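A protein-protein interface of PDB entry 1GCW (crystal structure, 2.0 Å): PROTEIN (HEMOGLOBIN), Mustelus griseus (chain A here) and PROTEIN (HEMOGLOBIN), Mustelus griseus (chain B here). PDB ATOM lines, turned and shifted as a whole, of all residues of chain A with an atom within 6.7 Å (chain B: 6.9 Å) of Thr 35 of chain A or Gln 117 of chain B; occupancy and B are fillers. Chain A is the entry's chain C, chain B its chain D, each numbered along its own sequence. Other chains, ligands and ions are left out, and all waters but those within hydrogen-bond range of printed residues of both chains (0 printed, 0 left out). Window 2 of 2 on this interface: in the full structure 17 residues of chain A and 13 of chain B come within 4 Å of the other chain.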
ATOM      1  N   GLU A  27      19.566  10.040  -0.014  1.00  0.00           N
ATOM      2  CA  GLU A  27      19.116  10.952   1.034  1.00  0.00           C
ATOM      3  C   GLU A  27      18.595  10.180   2.244  1.00  0.00           C
ATOM      4  O   GLU A  27      18.846  10.561   3.389  1.00  0.00           O
ATOM      5  CB  GLU A  27      18.022  11.873   0.502  1.00  0.00           C
ATOM      6  CG  GLU A  27      17.725  13.057   1.402  1.00  0.00           C
ATOM      7  CD  GLU A  27      16.653  13.963   0.824  1.00  0.00           C
ATOM      8  OE1 GLU A  27      16.578  14.075  -0.417  1.00  0.00           O
ATOM      9  OE2 GLU A  27      15.887  14.564   1.610  1.00  0.00           O
ATOM     10  N   ALA A  30      21.574   8.573   4.140  1.00  0.00           N
ATOM     11  CA  ALA A  30      22.329   9.644   4.777  1.00  0.00           C
ATOM     12  C   ALA A  30      21.624  10.141   6.040  1.00  0.00           C
ATOM     13  O   ALA A  30      22.264  10.397   7.066  1.00  0.00           O
ATOM     14  CB  ALA A  30      22.534  10.792   3.792  1.00  0.00           C
ATOM     15  N   ARG A  31      20.304  10.281   5.963  1.00  0.00           N
ATOM     16  CA  ARG A  31      19.528  10.732   7.112  1.00  0.00           C
ATOM     17  C   ARG A  31      19.646   9.680   8.208  1.00  0.00           C
ATOM     18  O   ARG A  31      19.800  10.001   9.390  1.00  0.00           O
ATOM     19  CB  ARG A  31      18.062  10.911   6.714  1.00  0.00           C
ATOM     20  CG  ARG A  31      17.781  12.224   6.006  1.00  0.00           C
ATOM     21  CD  ARG A  31      16.368  12.276   5.436  1.00  0.00           C
ATOM     22  NE  ARG A  31      16.141  13.508   4.688  1.00  0.00           N
ATOM     23  CZ  ARG A  31      16.158  14.724   5.220  1.00  0.00           C
ATOM     24  NH1 ARG A  31      15.944  15.781   4.453  1.00  0.00           N
ATOM     25  NH2 ARG A  31      16.384  14.890   6.516  1.00  0.00           N
ATOM     26  N   LEU A  32      19.579   8.419   7.794  1.00  0.00           N
ATOM     27  CA  LEU A  32      19.678   7.300   8.713  1.00  0.00           C
ATOM     28  C   LEU A  32      21.046   7.275   9.376  1.00  0.00           C
ATOM     29  O   LEU A  32      21.158   7.035  10.575  1.00  0.00           O
ATOM     30  CB  LEU A  32      19.464   5.984   7.969  1.00  0.00           C
ATOM     31  CG  LEU A  32      19.928   4.742   8.726  1.00  0.00           C
ATOM     32  CD1 LEU A  32      18.975   4.469   9.870  1.00  0.00           C
ATOM     33  CD2 LEU A  32      19.992   3.554   7.793  1.00  0.00           C
ATOM     34  N   PHE A  33      22.085   7.523   8.588  1.00  0.00           N
ATOM     35  CA  PHE A  33      23.442   7.508   9.114  1.00  0.00           C
ATOM     36  C   PHE A  33      23.692   8.643  10.102  1.00  0.00           C
ATOM     37  O   PHE A  33      24.378   8.455  11.108  1.00  0.00           O
ATOM     38  CB  PHE A  33      24.453   7.570   7.961  1.00  0.00           C
ATOM     39  CG  PHE A  33      24.528   6.301   7.140  1.00  0.00           C
ATOM     40  CD1 PHE A  33      24.679   6.356   5.756  1.00  0.00           C
ATOM     41  CD2 PHE A  33      24.435   5.054   7.746  1.00  0.00           C
ATOM     42  CE1 PHE A  33      24.734   5.189   4.989  1.00  0.00           C
ATOM     43  CE2 PHE A  33      24.489   3.884   6.985  1.00  0.00           C
ATOM     44  CZ  PHE A  33      24.638   3.957   5.601  1.00  0.00           C
ATOM     45  N   VAL A  34      23.127   9.816   9.829  1.00  0.00           N
ATOM     46  CA  VAL A  34      23.312  10.961  10.711  1.00  0.00           C
ATOM     47  C   VAL A  34      22.514  10.862  12.014  1.00  0.00           C
ATOM     48  O   VAL A  34      23.001  11.259  13.071  1.00  0.00           O
ATOM     49  CB  VAL A  34      22.930  12.279  10.003  1.00  0.00           C
ATOM     50  CG1 VAL A  34      22.732  13.391  11.030  1.00  0.00           C
ATOM     51  CG2 VAL A  34      24.013  12.671   9.020  1.00  0.00           C
ATOM     52  N   THR A  35      21.297  10.331  11.948  1.00  0.00           N
ATOM     53  CA  THR A  35      20.456  10.228  13.140  1.00  0.00           C
ATOM     54  C   THR A  35      20.714   8.993  13.997  1.00  0.00           C
ATOM     55  O   THR A  35      20.489   9.014  15.204  1.00  0.00           O
ATOM     56  CB  THR A  35      18.962  10.260  12.762  1.00  0.00           C
ATOM     57  OG1 THR A  35      18.694   9.272  11.759  1.00  0.00           O
ATOM     58  CG2 THR A  35      18.594  11.626  12.227  1.00  0.00           C
ATOM     59  N   HIS A  36      21.179   7.918  13.375  1.00  0.00           N
ATOM     60  CA  HIS A  36      21.464   6.687  14.100  1.00  0.00           C
ATOM     61  C   HIS A  36      22.804   6.100  13.679  1.00  0.00           C
ATOM     62  O   HIS A  36      22.862   5.056  13.028  1.00  0.00           O
ATOM     63  CB  HIS A  36      20.347   5.681  13.864  1.00  0.00           C
ATOM     64  CG  HIS A  36      19.005   6.189  14.281  1.00  0.00           C
ATOM     65  ND1 HIS A  36      18.534   6.070  15.571  1.00  0.00           N
ATOM     66  CD2 HIS A  36      18.055   6.867  13.594  1.00  0.00           C
ATOM     67  CE1 HIS A  36      17.352   6.653  15.660  1.00  0.00           C
ATOM     68  NE2 HIS A  36      17.039   7.144  14.474  1.00  0.00           N
ATOM     69  N   PRO A  37      23.901   6.768  14.073  1.00  0.00           N
ATOM     70  CA  PRO A  37      25.283   6.372  13.769  1.00  0.00           C
ATOM     71  C   PRO A  37      25.533   4.866  13.815  1.00  0.00           C
ATOM     72  O   PRO A  37      26.256   4.328  12.976  1.00  0.00           O
ATOM     73  CB  PRO A  37      26.102   7.121  14.811  1.00  0.00           C
ATOM     74  CG  PRO A  37      25.297   8.365  15.087  1.00  0.00           C
ATOM     75  CD  PRO A  37      23.848   7.994  14.898  1.00  0.00           C
ATOM     76  N   GLY A  38      24.928   4.192  14.789  1.00  0.00           N
ATOM     77  CA  GLY A  38      25.112   2.758  14.922  1.00  0.00           C
ATOM     78  C   GLY A  38      24.851   1.953  13.664  1.00  0.00           C
ATOM     79  O   GLY A  38      25.378   0.852  13.501  1.00  0.00           O
ATOM     80  N   SER A  39      24.040   2.493  12.763  1.00  0.00           N
ATOM     81  CA  SER A  39      23.712   1.788  11.528  1.00  0.00           C
ATOM     82  C   SER A  39      24.888   1.739  10.554  1.00  0.00           C
ATOM     83  O   SER A  39      24.981   0.833   9.721  1.00  0.00           O
ATOM     84  CB  SER A  39      22.508   2.451  10.861  1.00  0.00           C
ATOM     85  OG  SER A  39      22.618   3.861  10.944  1.00  0.00           O
ATOM     86  N   MET A 100      13.864   2.577  11.805  1.00  0.00           N
ATOM     87  CA  MET A 100      14.683   3.778  11.711  1.00  0.00           C
ATOM     88  C   MET A 100      14.846   4.195  10.250  1.00  0.00           C
ATOM     89  O   MET A 100      14.796   5.383   9.937  1.00  0.00           O
ATOM     90  CB  MET A 100      16.055   3.541  12.343  1.00  0.00           C
ATOM     91  CG  MET A 100      16.150   3.935  13.807  1.00  0.00           C
ATOM     92  SD  MET A 100      17.145   2.767  14.791  1.00  0.00           S
ATOM     93  CE  MET A 100      18.795   2.940  14.069  1.00  0.00           C
ATOM     94  N   GLU A 103      11.341   5.716   8.902  1.00  0.00           N
ATOM     95  CA  GLU A 103      11.092   7.113   9.228  1.00  0.00           C
ATOM     96  C   GLU A 103      11.939   8.033   8.356  1.00  0.00           C
ATOM     97  O   GLU A 103      11.503   9.117   7.963  1.00  0.00           O
ATOM     98  CB  GLU A 103      11.413   7.380  10.700  1.00  0.00           C
ATOM     99  CG  GLU A 103      10.197   7.562  11.615  1.00  0.00           C
ATOM    100  CD  GLU A 103       8.871   7.648  10.869  1.00  0.00           C
ATOM    101  OE1 GLU A 103       8.318   8.765  10.783  1.00  0.00           O
ATOM    102  OE2 GLU A 103       8.384   6.602  10.379  1.00  0.00           O
ATOM    103  N   CYS A 104      13.158   7.606   8.061  1.00  0.00           N
ATOM    104  CA  CYS A 104      14.047   8.411   7.240  1.00  0.00           C
ATOM    105  C   CYS A 104      13.491   8.493   5.825  1.00  0.00           C
ATOM    106  O   CYS A 104      13.588   9.534   5.185  1.00  0.00           O
ATOM    107  CB  CYS A 104      15.448   7.804   7.237  1.00  0.00           C
ATOM    108  SG  CYS A 104      16.363   8.180   8.738  1.00  0.00           S
ATOM    109  N   VAL A 107      10.531  10.837   6.190  1.00  0.00           N
ATOM    110  CA  VAL A 107      10.960  12.229   6.324  1.00  0.00           C
ATOM    111  C   VAL A 107      11.442  12.789   4.994  1.00  0.00           C
ATOM    112  O   VAL A 107      11.213  13.963   4.677  1.00  0.00           O
ATOM    113  CB  VAL A 107      12.104  12.374   7.348  1.00  0.00           C
ATOM    114  CG1 VAL A 107      12.683  13.785   7.286  1.00  0.00           C
ATOM    115  CG2 VAL A 107      11.589  12.084   8.750  1.00  0.00           C
ATOM    116  N   THR A 108      12.125  11.947   4.224  1.00  0.00           N
ATOM    117  CA  THR A 108      12.631  12.341   2.919  1.00  0.00           C
ATOM    118  C   THR A 108      11.455  12.696   2.009  1.00  0.00           C
ATOM    119  O   THR A 108      11.490  13.700   1.302  1.00  0.00           O
ATOM    120  CB  THR A 108      13.461  11.200   2.283  1.00  0.00           C
ATOM    121  OG1 THR A 108      14.651  10.988   3.057  1.00  0.00           O
ATOM    122  CG2 THR A 108      13.853  11.550   0.858  1.00  0.00           C
ATOM    123  N   ILE B 101       8.299  16.164  13.628  1.00  0.00           N
ATOM    124  CA  ILE B 101       9.462  16.239  12.753  1.00  0.00           C
ATOM    125  C   ILE B 101       8.984  16.201  11.308  1.00  0.00           C
ATOM    126  O   ILE B 101       9.467  16.958  10.468  1.00  0.00           O
ATOM    127  CB  ILE B 101      10.451  15.061  13.006  1.00  0.00           C
ATOM    128  CG1 ILE B 101      11.512  15.485  14.018  1.00  0.00           C
ATOM    129  CG2 ILE B 101      11.158  14.662  11.721  1.00  0.00           C
ATOM    130  CD1 ILE B 101      12.161  14.324  14.733  1.00  0.00           C
ATOM    131  N   PHE B 112      15.516  21.342   5.096  1.00  0.00           N
ATOM    132  CA  PHE B 112      15.525  20.392   6.213  1.00  0.00           C
ATOM    133  C   PHE B 112      16.496  19.247   5.900  1.00  0.00           C
ATOM    134  O   PHE B 112      16.095  18.092   5.742  1.00  0.00           O
ATOM    135  CB  PHE B 112      14.110  19.835   6.441  1.00  0.00           C
ATOM    136  CG  PHE B 112      13.881  19.290   7.826  1.00  0.00           C
ATOM    137  CD1 PHE B 112      13.649  20.151   8.900  1.00  0.00           C
ATOM    138  CD2 PHE B 112      13.897  17.912   8.061  1.00  0.00           C
ATOM    139  CE1 PHE B 112      13.438  19.649  10.194  1.00  0.00           C
ATOM    140  CE2 PHE B 112      13.687  17.397   9.350  1.00  0.00           C
ATOM    141  CZ  PHE B 112      13.456  18.269  10.418  1.00  0.00           C
ATOM    142  N   THR B 113      17.777  19.586   5.813  1.00  0.00           N
ATOM    143  CA  THR B 113      18.826  18.619   5.515  1.00  0.00           C
ATOM    144  C   THR B 113      19.005  17.575   6.623  1.00  0.00           C
ATOM    145  O   THR B 113      18.504  17.750   7.735  1.00  0.00           O
ATOM    146  CB  THR B 113      20.163  19.346   5.308  1.00  0.00           C
ATOM    147  OG1 THR B 113      20.577  19.944   6.545  1.00  0.00           O
ATOM    148  CG2 THR B 113      20.013  20.428   4.248  1.00  0.00           C
ATOM    149  N   PRO B 114      19.720  16.472   6.332  1.00  0.00           N
ATOM    150  CA  PRO B 114      19.919  15.449   7.367  1.00  0.00           C
ATOM    151  C   PRO B 114      20.530  16.064   8.619  1.00  0.00           C
ATOM    152  O   PRO B 114      20.251  15.643   9.748  1.00  0.00           O
ATOM    153  CB  PRO B 114      20.859  14.438   6.707  1.00  0.00           C
ATOM    154  CG  PRO B 114      20.673  14.642   5.239  1.00  0.00           C
ATOM    155  CD  PRO B 114      20.360  16.102   5.057  1.00  0.00           C
ATOM    156  N   HIS B 115      21.361  17.077   8.407  1.00  0.00           N
ATOM    157  CA  HIS B 115      22.019  17.755   9.509  1.00  0.00           C
ATOM    158  C   HIS B 115      20.995  18.396  10.445  1.00  0.00           C
ATOM    159  O   HIS B 115      21.008  18.152  11.651  1.00  0.00           O
ATOM    160  CB  HIS B 115      22.984  18.819   8.971  1.00  0.00           C
ATOM    161  CG  HIS B 115      23.836  19.446  10.030  1.00  0.00           C
ATOM    162  ND1 HIS B 115      23.653  20.743  10.461  1.00  0.00           N
ATOM    163  CD2 HIS B 115      24.845  18.940  10.777  1.00  0.00           C
ATOM    164  CE1 HIS B 115      24.512  21.008  11.430  1.00  0.00           C
ATOM    165  NE2 HIS B 115      25.246  19.930  11.641  1.00  0.00           N
ATOM    166  N   ILE B 116      20.113  19.218   9.882  1.00  0.00           N
ATOM    167  CA  ILE B 116      19.074  19.894  10.656  1.00  0.00           C
ATOM    168  C   ILE B 116      18.192  18.880  11.379  1.00  0.00           C
ATOM    169  O   ILE B 116      17.825  19.073  12.540  1.00  0.00           O
ATOM    170  CB  ILE B 116      18.173  20.757   9.747  1.00  0.00           C
ATOM    171  CG1 ILE B 116      19.029  21.724   8.934  1.00  0.00           C
ATOM    172  CG2 ILE B 116      17.162  21.527  10.585  1.00  0.00           C
ATOM    173  CD1 ILE B 116      19.885  22.619   9.781  1.00  0.00           C
ATOM    174  N   GLN B 117      17.849  17.803  10.679  1.00  0.00           N
ATOM    175  CA  GLN B 117      17.015  16.758  11.254  1.00  0.00           C
ATOM    176  C   GLN B 117      17.702  16.189  12.488  1.00  0.00           C
ATOM    177  O   GLN B 117      17.067  15.979  13.524  1.00  0.00           O
ATOM    178  CB  GLN B 117      16.781  15.644  10.231  1.00  0.00           C
ATOM    179  CG  GLN B 117      16.012  14.451  10.780  1.00  0.00           C
ATOM    180  CD  GLN B 117      15.911  13.315   9.784  1.00  0.00           C
ATOM    181  OE1 GLN B 117      16.244  13.471   8.611  1.00  0.00           O
ATOM    182  NE2 GLN B 117      15.450  12.161  10.250  1.00  0.00           N
ATOM    183  N   GLY B 118      19.008  15.950  12.365  1.00  0.00           N
ATOM    184  CA  GLY B 118      19.777  15.408  13.469  1.00  0.00           C
ATOM    185  C   GLY B 118      19.669  16.261  14.715  1.00  0.00           C
ATOM    186  O   GLY B 118      19.674  15.748  15.835  1.00  0.00           O
ATOM    187  N   ILE B 119      19.568  17.572  14.524  1.00  0.00           N
ATOM    188  CA  ILE B 119      19.456  18.492  15.649  1.00  0.00           C
ATOM    189  C   ILE B 119      18.135  18.292  16.382  1.00  0.00           C
ATOM    190  O   ILE B 119      18.098  18.137  17.605  1.00  0.00           O
ATOM    191  CB  ILE B 119      19.535  19.959  15.182  1.00  0.00           C
ATOM    192  CG1 ILE B 119      20.945  20.270  14.673  1.00  0.00           C
ATOM    193  CG2 ILE B 119      19.154  20.888  16.332  1.00  0.00           C
ATOM    194  CD1 ILE B 119      21.146  21.714  14.286  1.00  0.00           C
ATOM    195  N   TRP B 120      17.051  18.303  15.616  1.00  0.00           N
ATOM    196  CA  TRP B 120      15.718  18.125  16.164  1.00  0.00           C
ATOM    197  C   TRP B 120      15.546  16.750  16.783  1.00  0.00           C
ATOM    198  O   TRP B 120      14.909  16.607  17.826  1.00  0.00           O
ATOM    199  CB  TRP B 120      14.691  18.346  15.068  1.00  0.00           C
ATOM    200  CG  TRP B 120      14.524  19.779  14.810  1.00  0.00           C
ATOM    201  CD1 TRP B 120      15.081  20.499  13.800  1.00  0.00           C
ATOM    202  CD2 TRP B 120      13.828  20.711  15.638  1.00  0.00           C
ATOM    203  NE1 TRP B 120      14.782  21.832  13.949  1.00  0.00           N
ATOM    204  CE2 TRP B 120      14.011  21.989  15.072  1.00  0.00           C
ATOM    205  CE3 TRP B 120      13.068  20.591  16.807  1.00  0.00           C
ATOM    206  CZ2 TRP B 120      13.459  23.145  15.638  1.00  0.00           C
ATOM    207  CZ3 TRP B 120      12.521  21.738  17.371  1.00  0.00           C
ATOM    208  CH2 TRP B 120      12.719  22.998  16.784  1.00  0.00           C
ATOM    209  N   ASP B 121      16.121  15.743  16.132  1.00  0.00           N
ATOM    210  CA  ASP B 121      16.057  14.372  16.618  1.00  0.00           C
ATOM    211  C   ASP B 121      16.704  14.328  17.997  1.00  0.00           C
ATOM    212  O   ASP B 121      16.254  13.607  18.888  1.00  0.00           O
ATOM    213  CB  ASP B 121      16.809  13.448  15.659  1.00  0.00           C
ATOM    214  CG  ASP B 121      16.514  11.987  15.907  1.00  0.00           C
ATOM    215  OD1 ASP B 121      17.066  11.425  16.875  1.00  0.00           O
ATOM    216  OD2 ASP B 121      15.733  11.398  15.132  1.00  0.00           O
ATOM    217  N   LYS B 122      17.762  15.116  18.163  1.00  0.00           N
ATOM    218  CA  LYS B 122      18.482  15.184  19.424  1.00  0.00           C
ATOM    219  C   LYS B 122      17.609  15.865  20.459  1.00  0.00           C
ATOM    220  O   LYS B 122      17.435  15.362  21.574  1.00  0.00           O
ATOM    221  CB  LYS B 122      19.778  15.978  19.252  1.00  0.00           C
ATOM    222  CG  LYS B 122      20.759  15.811  20.401  1.00  0.00           C
ATOM    223  CD  LYS B 122      21.498  17.106  20.698  1.00  0.00           C
ATOM    224  CE  LYS B 122      22.357  16.979  21.955  1.00  0.00           C
ATOM    225  NZ  LYS B 122      23.576  17.842  21.902  1.00  0.00           N
ATOM    226  N   PHE B 123      17.062  17.015  20.079  1.00  0.00           N
ATOM    227  CA  PHE B 123      16.206  17.778  20.972  1.00  0.00           C
ATOM    228  C   PHE B 123      15.088  16.900  21.503  1.00  0.00           C
ATOM    229  O   PHE B 123      14.871  16.817  22.714  1.00  0.00           O
ATOM    230  CB  PHE B 123      15.600  18.976  20.242  1.00  0.00           C
ATOM    231  CG  PHE B 123      14.565  19.711  21.051  1.00  0.00           C
ATOM    232  CD1 PHE B 123      14.907  20.323  22.254  1.00  0.00           C
ATOM    233  CD2 PHE B 123      13.234  19.754  20.639  1.00  0.00           C
ATOM    234  CE1 PHE B 123      13.937  20.959  23.035  1.00  0.00           C
ATOM    235  CE2 PHE B 123      12.258  20.389  21.413  1.00  0.00           C
ATOM    236  CZ  PHE B 123      12.611  20.989  22.610  1.00  0.00           C
ATOM    237  N   GLU B 125      14.830  13.561  21.330  1.00  0.00           N
ATOM    238  CA  GLU B 125      15.297  12.352  21.987  1.00  0.00           C
ATOM    239  C   GLU B 125      15.523  12.683  23.452  1.00  0.00           C
ATOM    240  O   GLU B 125      15.406  11.820  24.323  1.00  0.00           O
ATOM    241  CB  GLU B 125      16.597  11.885  21.363  1.00  0.00           C
ATOM    242  CG  GLU B 125      16.699  10.392  21.217  1.00  0.00           C
ATOM    243  CD  GLU B 125      18.043   9.985  20.665  1.00  0.00           C
ATOM    244  OE1 GLU B 125      18.164   9.874  19.424  1.00  0.00           O
ATOM    245  OE2 GLU B 125      18.981   9.784  21.469  1.00  0.00           O
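The guanidinium group (NH1) of Arg 31 of chain A sits at hydrogen-bond distance from the backbone carbonyl oxygen (O) of Phe 112 of chain B (2.7 Å).
NH2 of Arg 31 of chain A lies within hydrogen-bond range of OE1 of Gln 117 of chain B (2.5 Å).
Phe 33 of chain A touches none of the printed residues of chain B.
Thr 35 of chain A touches just one residue of chain B: Gln 117 (3.8 Å).
Cys 104 of chain A touches none of the printed residues of chain B.
Printed residues of chain A within 4 Å of Phe 112 of chain B: Arg 31.
Printed residues of chain A within 4 Å of Thr 113 of chain B: Arg 31.
Of the printed residues of chain A, Pro 114 of chain B touches Arg 31 (3.7 Å) and Val 34 (3.6 Å).
Gln 117 of chain B touches three residues of chain A.
The nearest residue of chain A that does not touch Gln 117 of chain B is Cys 104 of chain A (4.4 Å).
Of the 16 printed residues of chain A, 4 touch a printed residue of chain B.
Printed residues of chain A that touch a printed residue of chain B: Arg 31, Val 34, Thr 35 and Val 107.
Hydrophobic or aromatic side chains of chain A that line the printed part of chain B: Val 34 and Val 107.
Of the 14 printed residues of chain B, 5 touch a printed residue of chain A.
C of Thr 113 of chain B touches NH2 of Arg 31 of chain A, at 3.8 Å.
Pro 114 of chain B touches Arg 31 of chain A (CA to NH2, 3.7 Å).
Val 34 of chain A touches Pro 114 of chain B.
CG2 of Thr 35 of chain A touches NE2 of Gln 117 of chain B, 3.8 Å away.
CG2 of Val 107 of chain A touches CG2 of Ile 101 of chain B, at 3.96 Å.
OE1 of Gln 117 of chain B touches CG1 of Val 107 of chain A, 3.8 Å away.
The side-chain carboxylate (OE2) of Glu 27 of chain A lies within salt-bridge range of the guanidinium group (NH1) of Arg 31 of chain A, 3.1 Å away.
The backbone carbonyl oxygen of Arg 31 of chain A sits at hydrogen-bond distance from the side-chain hydroxyl of Thr 35 of chain A.
The guanidinium group of Arg 31 of chain A sits close to the side-chain hydroxyl of Thr 108 of chain A (3.4 Å).
The backbone NH of Ile 116 of chain B sits close to the side-chain hydroxyl of Thr 113 of chain B.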
